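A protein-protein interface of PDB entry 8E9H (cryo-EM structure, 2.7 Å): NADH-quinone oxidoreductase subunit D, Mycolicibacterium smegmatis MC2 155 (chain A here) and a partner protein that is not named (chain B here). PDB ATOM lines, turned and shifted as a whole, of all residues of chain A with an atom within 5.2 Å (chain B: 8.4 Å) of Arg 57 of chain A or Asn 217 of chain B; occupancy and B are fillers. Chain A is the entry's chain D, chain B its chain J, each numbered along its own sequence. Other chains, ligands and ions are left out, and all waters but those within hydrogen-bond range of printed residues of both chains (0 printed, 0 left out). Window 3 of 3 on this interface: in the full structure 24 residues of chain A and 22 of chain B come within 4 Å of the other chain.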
ATOM      1  N   ASN A  44     -16.107   1.124 -10.818  1.00  0.00           N
ATOM      2  CA  ASN A  44     -15.494   1.955 -11.843  1.00  0.00           C
ATOM      3  C   ASN A  44     -16.596   2.638 -12.634  1.00  0.00           C
ATOM      4  O   ASN A  44     -17.268   2.000 -13.447  1.00  0.00           O
ATOM      5  CB  ASN A  44     -14.621   1.114 -12.765  1.00  0.00           C
ATOM      6  CG  ASN A  44     -13.518   0.406 -12.030  1.00  0.00           C
ATOM      7  OD1 ASN A  44     -12.411   0.923 -11.907  1.00  0.00           O
ATOM      8  ND2 ASN A  44     -13.813  -0.783 -11.529  1.00  0.00           N
ATOM      9  N   MET A  45     -16.789   3.936 -12.403  1.00  0.00           N
ATOM     10  CA  MET A  45     -17.579   4.708 -13.350  1.00  0.00           C
ATOM     11  C   MET A  45     -16.939   4.597 -14.723  1.00  0.00           C
ATOM     12  O   MET A  45     -17.598   4.777 -15.752  1.00  0.00           O
ATOM     13  CB  MET A  45     -17.670   6.162 -12.902  1.00  0.00           C
ATOM     14  CG  MET A  45     -18.576   7.024 -13.750  1.00  0.00           C
ATOM     15  SD  MET A  45     -20.296   6.508 -13.689  1.00  0.00           S
ATOM     16  CE  MET A  45     -20.744   7.036 -12.041  1.00  0.00           C
ATOM     17  N   GLY A  46     -15.638   4.328 -14.746  1.00  0.00           N
ATOM     18  CA  GLY A  46     -14.990   3.673 -15.852  1.00  0.00           C
ATOM     19  C   GLY A  46     -14.889   4.515 -17.099  1.00  0.00           C
ATOM     20  O   GLY A  46     -15.643   5.470 -17.295  1.00  0.00           O
ATOM     21  N   PRO A  47     -13.949   4.171 -17.972  1.00  0.00           N
ATOM     22  CA  PRO A  47     -13.833   4.903 -19.233  1.00  0.00           C
ATOM     23  C   PRO A  47     -15.085   4.759 -20.074  1.00  0.00           C
ATOM     24  O   PRO A  47     -15.687   5.756 -20.478  1.00  0.00           O
ATOM     25  CB  PRO A  47     -12.615   4.259 -19.906  1.00  0.00           C
ATOM     26  CG  PRO A  47     -11.880   3.592 -18.813  1.00  0.00           C
ATOM     27  CD  PRO A  47     -12.908   3.139 -17.847  1.00  0.00           C
ATOM     28  N   VAL A  55     -13.329   8.111 -21.847  1.00  0.00           N
ATOM     29  CA  VAL A  55     -11.928   7.909 -21.489  1.00  0.00           C
ATOM     30  C   VAL A  55     -11.590   8.481 -20.119  1.00  0.00           C
ATOM     31  O   VAL A  55     -10.415   8.688 -19.804  1.00  0.00           O
ATOM     32  CB  VAL A  55     -11.006   8.518 -22.557  1.00  0.00           C
ATOM     33  CG1 VAL A  55     -11.200   7.816 -23.880  1.00  0.00           C
ATOM     34  CG2 VAL A  55     -11.256   9.998 -22.684  1.00  0.00           C
ATOM     35  N   LEU A  56     -12.598   8.746 -19.302  1.00  0.00           N
ATOM     36  CA  LEU A  56     -12.390   9.203 -17.934  1.00  0.00           C
ATOM     37  C   LEU A  56     -12.813   8.089 -16.989  1.00  0.00           C
ATOM     38  O   LEU A  56     -13.907   7.537 -17.138  1.00  0.00           O
ATOM     39  CB  LEU A  56     -13.187  10.477 -17.664  1.00  0.00           C
ATOM     40  CG  LEU A  56     -13.226  10.947 -16.215  1.00  0.00           C
ATOM     41  CD1 LEU A  56     -11.823  11.169 -15.695  1.00  0.00           C
ATOM     42  CD2 LEU A  56     -14.043  12.212 -16.100  1.00  0.00           C
ATOM     43  N   ARG A  57     -11.958   7.752 -16.023  1.00  0.00           N
ATOM     44  CA  ARG A  57     -12.267   6.641 -15.121  1.00  0.00           C
ATOM     45  C   ARG A  57     -12.529   7.175 -13.722  1.00  0.00           C
ATOM     46  O   ARG A  57     -11.616   7.373 -12.934  1.00  0.00           O
ATOM     47  CB  ARG A  57     -11.137   5.623 -15.115  1.00  0.00           C
ATOM     48  CG  ARG A  57     -11.424   4.412 -14.256  1.00  0.00           C
ATOM     49  CD  ARG A  57     -10.239   3.485 -14.205  1.00  0.00           C
ATOM     50  NE  ARG A  57     -10.459   2.377 -13.287  1.00  0.00           N
ATOM     51  CZ  ARG A  57      -9.519   1.527 -12.905  1.00  0.00           C
ATOM     52  NH1 ARG A  57      -8.277   1.624 -13.349  1.00  0.00           N
ATOM     53  NH2 ARG A  57      -9.830   0.556 -12.054  1.00  0.00           N
ATOM     54  N   LEU A  58     -13.794   7.385 -13.389  1.00  0.00           N
ATOM     55  CA  LEU A  58     -14.131   7.716 -12.013  1.00  0.00           C
ATOM     56  C   LEU A  58     -14.299   6.439 -11.201  1.00  0.00           C
ATOM     57  O   LEU A  58     -15.233   5.666 -11.426  1.00  0.00           O
ATOM     58  CB  LEU A  58     -15.401   8.558 -11.962  1.00  0.00           C
ATOM     59  CG  LEU A  58     -15.192  10.064 -11.895  1.00  0.00           C
ATOM     60  CD1 LEU A  58     -14.695  10.590 -13.216  1.00  0.00           C
ATOM     61  CD2 LEU A  58     -16.488  10.741 -11.513  1.00  0.00           C
ATOM     62  N   ILE A  59     -13.382   6.208 -10.267  1.00  0.00           N
ATOM     63  CA  ILE A  59     -13.461   5.089  -9.337  1.00  0.00           C
ATOM     64  C   ILE A  59     -14.158   5.600  -8.088  1.00  0.00           C
ATOM     65  O   ILE A  59     -13.599   6.420  -7.352  1.00  0.00           O
ATOM     66  CB  ILE A  59     -12.075   4.525  -8.996  1.00  0.00           C
ATOM     67  CG1 ILE A  59     -11.327   4.142 -10.271  1.00  0.00           C
ATOM     68  CG2 ILE A  59     -12.203   3.324  -8.081  1.00  0.00           C
ATOM     69  CD1 ILE A  59     -10.363   5.194 -10.738  1.00  0.00           C
ATOM     70  N   ARG A  71     -11.933   8.766  -6.968  1.00  0.00           N
ATOM     71  CA  ARG A  71     -10.609   8.817  -7.563  1.00  0.00           C
ATOM     72  C   ARG A  71     -10.776   8.914  -9.070  1.00  0.00           C
ATOM     73  O   ARG A  71     -11.813   8.529  -9.610  1.00  0.00           O
ATOM     74  CB  ARG A  71      -9.780   7.578  -7.226  1.00  0.00           C
ATOM     75  CG  ARG A  71      -9.544   7.342  -5.751  1.00  0.00           C
ATOM     76  CD  ARG A  71      -8.832   6.016  -5.540  1.00  0.00           C
ATOM     77  NE  ARG A  71      -8.167   5.942  -4.247  1.00  0.00           N
ATOM     78  CZ  ARG A  71      -8.796   5.799  -3.089  1.00  0.00           C
ATOM     79  NH1 ARG A  71     -10.113   5.706  -3.025  1.00  0.00           N
ATOM     80  NH2 ARG A  71      -8.085   5.745  -1.968  1.00  0.00           N
ATOM     81  N   CYS A  72      -9.755   9.421  -9.753  1.00  0.00           N
ATOM     82  CA  CYS A  72      -9.799   9.566 -11.203  1.00  0.00           C
ATOM     83  C   CYS A  72      -8.608   8.887 -11.856  1.00  0.00           C
ATOM     84  O   CYS A  72      -7.471   9.344 -11.719  1.00  0.00           O
ATOM     85  CB  CYS A  72      -9.847  11.034 -11.610  1.00  0.00           C
ATOM     86  SG  CYS A  72     -11.361  11.830 -11.144  1.00  0.00           S
ATOM     87  N   GLY A  73      -8.884   7.801 -12.571  1.00  0.00           N
ATOM     88  CA  GLY A  73      -7.960   7.300 -13.554  1.00  0.00           C
ATOM     89  C   GLY A  73      -8.012   8.155 -14.808  1.00  0.00           C
ATOM     90  O   GLY A  73      -9.045   8.272 -15.474  1.00  0.00           O
ATOM     91  N   TYR A  76      -6.255   7.607 -20.086  1.00  0.00           N
ATOM     92  CA  TYR A  76      -6.784   6.680 -21.071  1.00  0.00           C
ATOM     93  C   TYR A  76      -6.851   7.307 -22.450  1.00  0.00           C
ATOM     94  O   TYR A  76      -6.951   6.581 -23.443  1.00  0.00           O
ATOM     95  CB  TYR A  76      -8.161   6.199 -20.631  1.00  0.00           C
ATOM     96  CG  TYR A  76      -8.087   5.347 -19.396  1.00  0.00           C
ATOM     97  CD1 TYR A  76      -7.772   4.003 -19.476  1.00  0.00           C
ATOM     98  CD2 TYR A  76      -8.304   5.894 -18.145  1.00  0.00           C
ATOM     99  CE1 TYR A  76      -7.689   3.227 -18.348  1.00  0.00           C
ATOM    100  CE2 TYR A  76      -8.222   5.126 -17.013  1.00  0.00           C
ATOM    101  CZ  TYR A  76      -7.915   3.794 -17.119  1.00  0.00           C
ATOM    102  OH  TYR A  76      -7.834   3.026 -15.985  1.00  0.00           O
ATOM    103  N   ASN B 209      -5.220   7.401  -8.095  1.00  0.00           N
ATOM    104  CA  ASN B 209      -5.957   6.348  -8.759  1.00  0.00           C
ATOM    105  C   ASN B 209      -5.302   5.003  -8.479  1.00  0.00           C
ATOM    106  O   ASN B 209      -4.108   4.929  -8.190  1.00  0.00           O
ATOM    107  CB  ASN B 209      -5.998   6.605 -10.262  1.00  0.00           C
ATOM    108  CG  ASN B 209      -4.613   6.673 -10.873  1.00  0.00           C
ATOM    109  OD1 ASN B 209      -3.611   6.532 -10.175  1.00  0.00           O
ATOM    110  ND2 ASN B 209      -4.548   6.887 -12.178  1.00  0.00           N
ATOM    111  N   PRO B 210      -6.059   3.914  -8.549  1.00  0.00           N
ATOM    112  CA  PRO B 210      -5.438   2.592  -8.486  1.00  0.00           C
ATOM    113  C   PRO B 210      -4.520   2.375  -9.675  1.00  0.00           C
ATOM    114  O   PRO B 210      -4.757   2.867 -10.779  1.00  0.00           O
ATOM    115  CB  PRO B 210      -6.628   1.633  -8.513  1.00  0.00           C
ATOM    116  CG  PRO B 210      -7.721   2.404  -9.137  1.00  0.00           C
ATOM    117  CD  PRO B 210      -7.517   3.823  -8.719  1.00  0.00           C
ATOM    118  N   GLY B 211      -3.452   1.625  -9.432  1.00  0.00           N
ATOM    119  CA  GLY B 211      -2.451   1.381 -10.452  1.00  0.00           C
ATOM    120  C   GLY B 211      -3.045   0.659 -11.650  1.00  0.00           C
ATOM    121  O   GLY B 211      -3.896  -0.214 -11.508  1.00  0.00           O
ATOM    122  N   VAL B 212      -2.588   1.047 -12.834  1.00  0.00           N
ATOM    123  CA  VAL B 212      -2.997   0.422 -14.083  1.00  0.00           C
ATOM    124  C   VAL B 212      -1.779  -0.287 -14.650  1.00  0.00           C
ATOM    125  O   VAL B 212      -0.845   0.359 -15.139  1.00  0.00           O
ATOM    126  CB  VAL B 212      -3.556   1.442 -15.080  1.00  0.00           C
ATOM    127  CG1 VAL B 212      -3.865   0.768 -16.398  1.00  0.00           C
ATOM    128  CG2 VAL B 212      -4.800   2.094 -14.518  1.00  0.00           C
ATOM    129  N   TYR B 213      -1.784  -1.609 -14.582  1.00  0.00           N
ATOM    130  CA  TYR B 213      -0.719  -2.432 -15.127  1.00  0.00           C
ATOM    131  C   TYR B 213      -1.266  -3.242 -16.288  1.00  0.00           C
ATOM    132  O   TYR B 213      -2.464  -3.526 -16.347  1.00  0.00           O
ATOM    133  CB  TYR B 213      -0.148  -3.384 -14.075  1.00  0.00           C
ATOM    134  CG  TYR B 213       0.366  -2.706 -12.833  1.00  0.00           C
ATOM    135  CD1 TYR B 213      -0.499  -2.100 -11.941  1.00  0.00           C
ATOM    136  CD2 TYR B 213       1.719  -2.681 -12.549  1.00  0.00           C
ATOM    137  CE1 TYR B 213      -0.033  -1.484 -10.806  1.00  0.00           C
ATOM    138  CE2 TYR B 213       2.194  -2.065 -11.416  1.00  0.00           C
ATOM    139  CZ  TYR B 213       1.313  -1.469 -10.547  1.00  0.00           C
ATOM    140  OH  TYR B 213       1.778  -0.853  -9.411  1.00  0.00           O
ATOM    141  N   ALA B 214      -0.392  -3.605 -17.219  1.00  0.00           N
ATOM    142  CA  ALA B 214      -0.763  -4.619 -18.185  1.00  0.00           C
ATOM    143  C   ALA B 214      -1.130  -5.890 -17.440  1.00  0.00           C
ATOM    144  O   ALA B 214      -0.394  -6.346 -16.562  1.00  0.00           O
ATOM    145  CB  ALA B 214       0.387  -4.883 -19.156  1.00  0.00           C
ATOM    146  N   ARG B 215      -2.280  -6.457 -17.783  1.00  0.00           N
ATOM    147  CA  ARG B 215      -2.877  -7.642 -17.183  1.00  0.00           C
ATOM    148  C   ARG B 215      -3.612  -7.324 -15.887  1.00  0.00           C
ATOM    149  O   ARG B 215      -4.221  -8.220 -15.310  1.00  0.00           O
ATOM    150  CB  ARG B 215      -1.853  -8.756 -16.902  1.00  0.00           C
ATOM    151  CG  ARG B 215      -1.046  -9.185 -18.103  1.00  0.00           C
ATOM    152  CD  ARG B 215      -0.121 -10.327 -17.748  1.00  0.00           C
ATOM    153  NE  ARG B 215       0.699 -10.735 -18.880  1.00  0.00           N
ATOM    154  CZ  ARG B 215       1.659 -11.645 -18.818  1.00  0.00           C
ATOM    155  NH1 ARG B 215       1.945 -12.272 -17.689  1.00  0.00           N
ATOM    156  NH2 ARG B 215       2.352 -11.933 -19.914  1.00  0.00           N
ATOM    157  N   HIS B 216      -3.582  -6.081 -15.411  1.00  0.00           N
ATOM    158  CA  HIS B 216      -4.232  -5.747 -14.146  1.00  0.00           C
ATOM    159  C   HIS B 216      -4.590  -4.272 -14.151  1.00  0.00           C
ATOM    160  O   HIS B 216      -3.697  -3.423 -14.140  1.00  0.00           O
ATOM    161  CB  HIS B 216      -3.325  -6.065 -12.958  1.00  0.00           C
ATOM    162  CG  HIS B 216      -2.987  -7.514 -12.825  1.00  0.00           C
ATOM    163  ND1 HIS B 216      -3.922  -8.467 -12.492  1.00  0.00           N
ATOM    164  CD2 HIS B 216      -1.813  -8.173 -12.971  1.00  0.00           C
ATOM    165  CE1 HIS B 216      -3.343  -9.653 -12.446  1.00  0.00           C
ATOM    166  NE2 HIS B 216      -2.062  -9.502 -12.732  1.00  0.00           N
ATOM    167  N   ASN B 217      -5.887  -3.970 -14.157  1.00  0.00           N
ATOM    168  CA  ASN B 217      -6.333  -2.589 -14.026  1.00  0.00           C
ATOM    169  C   ASN B 217      -7.534  -2.453 -13.099  1.00  0.00           C
ATOM    170  O   ASN B 217      -8.167  -1.391 -13.088  1.00  0.00           O
ATOM    171  CB  ASN B 217      -6.666  -1.997 -15.398  1.00  0.00           C
ATOM    172  CG  ASN B 217      -7.719  -2.789 -16.131  1.00  0.00           C
ATOM    173  OD1 ASN B 217      -8.505  -3.509 -15.524  1.00  0.00           O
ATOM    174  ND2 ASN B 217      -7.747  -2.651 -17.449  1.00  0.00           N
ATOM    175  N   SER B 218      -7.865  -3.478 -12.322  1.00  0.00           N
ATOM    176  CA  SER B 218      -8.974  -3.378 -11.391  1.00  0.00           C
ATOM    177  C   SER B 218      -8.661  -2.356 -10.304  1.00  0.00           C
ATOM    178  O   SER B 218      -7.524  -1.911 -10.140  1.00  0.00           O
ATOM    179  CB  SER B 218      -9.265  -4.737 -10.762  1.00  0.00           C
ATOM    180  OG  SER B 218      -8.077  -5.317 -10.257  1.00  0.00           O
ATOM    181  N   VAL B 219      -9.693  -1.983  -9.554  1.00  0.00           N
ATOM    182  CA  VAL B 219      -9.553  -0.972  -8.512  1.00  0.00           C
ATOM    183  C   VAL B 219      -8.751  -1.535  -7.349  1.00  0.00           C
ATOM    184  O   VAL B 219      -8.271  -0.786  -6.494  1.00  0.00           O
ATOM    185  CB  VAL B 219     -10.927  -0.472  -8.034  1.00  0.00           C
ATOM    186  CG1 VAL B 219     -11.699   0.129  -9.187  1.00  0.00           C
ATOM    187  CG2 VAL B 219     -11.710  -1.598  -7.392  1.00  0.00           C
ATOM    188  N   ASP B 220      -8.605  -2.857  -7.302  1.00  0.00           N
ATOM    189  CA  ASP B 220      -7.858  -3.493  -6.227  1.00  0.00           C
ATOM    190  C   ASP B 220      -6.358  -3.284  -6.369  1.00  0.00           C
ATOM    191  O   ASP B 220      -5.634  -3.299  -5.370  1.00  0.00           O
ATOM    192  CB  ASP B 220      -8.167  -4.990  -6.191  1.00  0.00           C
ATOM    193  N   VAL B 221      -5.879  -3.088  -7.593  1.00  0.00           N
ATOM    194  CA  VAL B 221      -4.449  -2.997  -7.867  1.00  0.00           C
ATOM    195  C   VAL B 221      -3.889  -1.728  -7.237  1.00  0.00           C
ATOM    196  O   VAL B 221      -4.500  -0.659  -7.366  1.00  0.00           O
ATOM    197  CB  VAL B 221      -4.178  -3.017  -9.377  1.00  0.00           C
ATOM    198  CG1 VAL B 221      -2.697  -2.952  -9.640  1.00  0.00           C
ATOM    199  CG2 VAL B 221      -4.775  -4.259 -10.007  1.00  0.00           C
ATOM    200  N   PRO B 222      -2.745  -1.786  -6.553  1.00  0.00           N
ATOM    201  CA  PRO B 222      -2.151  -0.563  -6.005  1.00  0.00           C
ATOM    202  C   PRO B 222      -1.197   0.110  -6.980  1.00  0.00           C
ATOM    203  O   PRO B 222      -0.495  -0.538  -7.757  1.00  0.00           O
ATOM    204  CB  PRO B 222      -1.403  -1.083  -4.773  1.00  0.00           C
ATOM    205  CG  PRO B 222      -0.958  -2.433  -5.180  1.00  0.00           C
ATOM    206  CD  PRO B 222      -2.021  -2.985  -6.101  1.00  0.00           C
ATOM    207  N   THR B 243      -4.173  -8.335  -6.044  1.00  0.00           N
ATOM    208  CA  THR B 243      -4.239  -8.020  -7.465  1.00  0.00           C
ATOM    209  C   THR B 243      -3.011  -7.231  -7.901  1.00  0.00           C
ATOM    210  O   THR B 243      -2.255  -7.669  -8.768  1.00  0.00           O
ATOM    211  CB  THR B 243      -5.503  -7.214  -7.808  1.00  0.00           C
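NH2 of Arg 57 of chain A lies within hydrogen-bond range of O of Asn 217 of chain B (2.8 Å).
The guanidinium group (NH2) of Arg 57 of chain A lies within hydrogen-bond range of the side-chain amide oxygen (OD1) of Asn 44 of chain A.
The backbone carbonyl oxygen of Arg 57 of chain A sits at hydrogen-bond distance from the backbone NH of Gly 73 of chain A, 2.8 Å away.
The side-chain hydroxyl of Tyr 76 of chain A sits at hydrogen-bond distance from the guanidinium group of Arg 57 of chain A (3.0 Å).
The backbone NH (N) of Ile 59 of chain A is in hydrogen-bond range of the backbone carbonyl oxygen (O) of Arg 71 of chain A (2.9 Å).
Asn 44 of chain A touches Val 219 of chain B.
CG2 of Val 212 of chain B touches NH1 of Arg 57 of chain A (3.7 Å).
Arg 57 of chain A touches Ser 218 of chain B.
Arg 57 of chain A touches Val 219 of chain B.
Ile 59 of chain A touches Pro 210 of chain B (CD1 to CD, 3.7 Å).
Val 219 of chain B touches Ile 59 of chain A.
Cys 72 of chain A touches Asn 209 of chain B (O to CB, 3.4 Å).
Gly 73 of chain A touches Asn 209 of chain B.
Tyr 76 of chain A touches Val 212 of chain B (OH to CG2, 3.5 Å).
Arg 57 of chain A touches just these residues of chain B: Val 212 (3.7 Å), Asn 217 (2.8 Å), Ser 218 (3.6 Å) and Val 219 (3.4 Å).
Asn 217 of chain B touches just one residue of chain A: Arg 57.
No residue of chain B comes within 4 Å of Gly 46 of chain A.
Printed residues of chain B within 4 Å of Gly 73 of chain A: Asn 209 (3.7 Å).
Printed residues of chain A within 4 Å of Val 219 of chain B: Asn 44, Arg 57 and Ile 59.
Of the printed residues of chain B, Cys 72 of chain A touches Asn 209.
Leu 56 of chain A touches none of the printed residues of chain B.
The nearest residue of chain B that does not touch Arg 57 of chain A is Pro 210 of chain B (4.05 Å).
The nearest printed residue of chain A that does not touch Asn 209 of chain B is Arg 71 of chain A (4.3 Å).
Of the 15 printed residues of chain B, 6 touch a printed residue of chain A.
Printed residues of chain B that touch a printed residue of chain A: Asn 209, Pro 210, Val 212, Asn 217, Ser 218 and Val 219.
Of the 13 printed residues of chain A, 6 touch a printed residue of chain B.
Hydrophobic or aromatic side chains of chain A that line the printed part of chain B: Ile 59 and Tyr 76.
Among the printed residues, 10 pairs touch across the chains.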
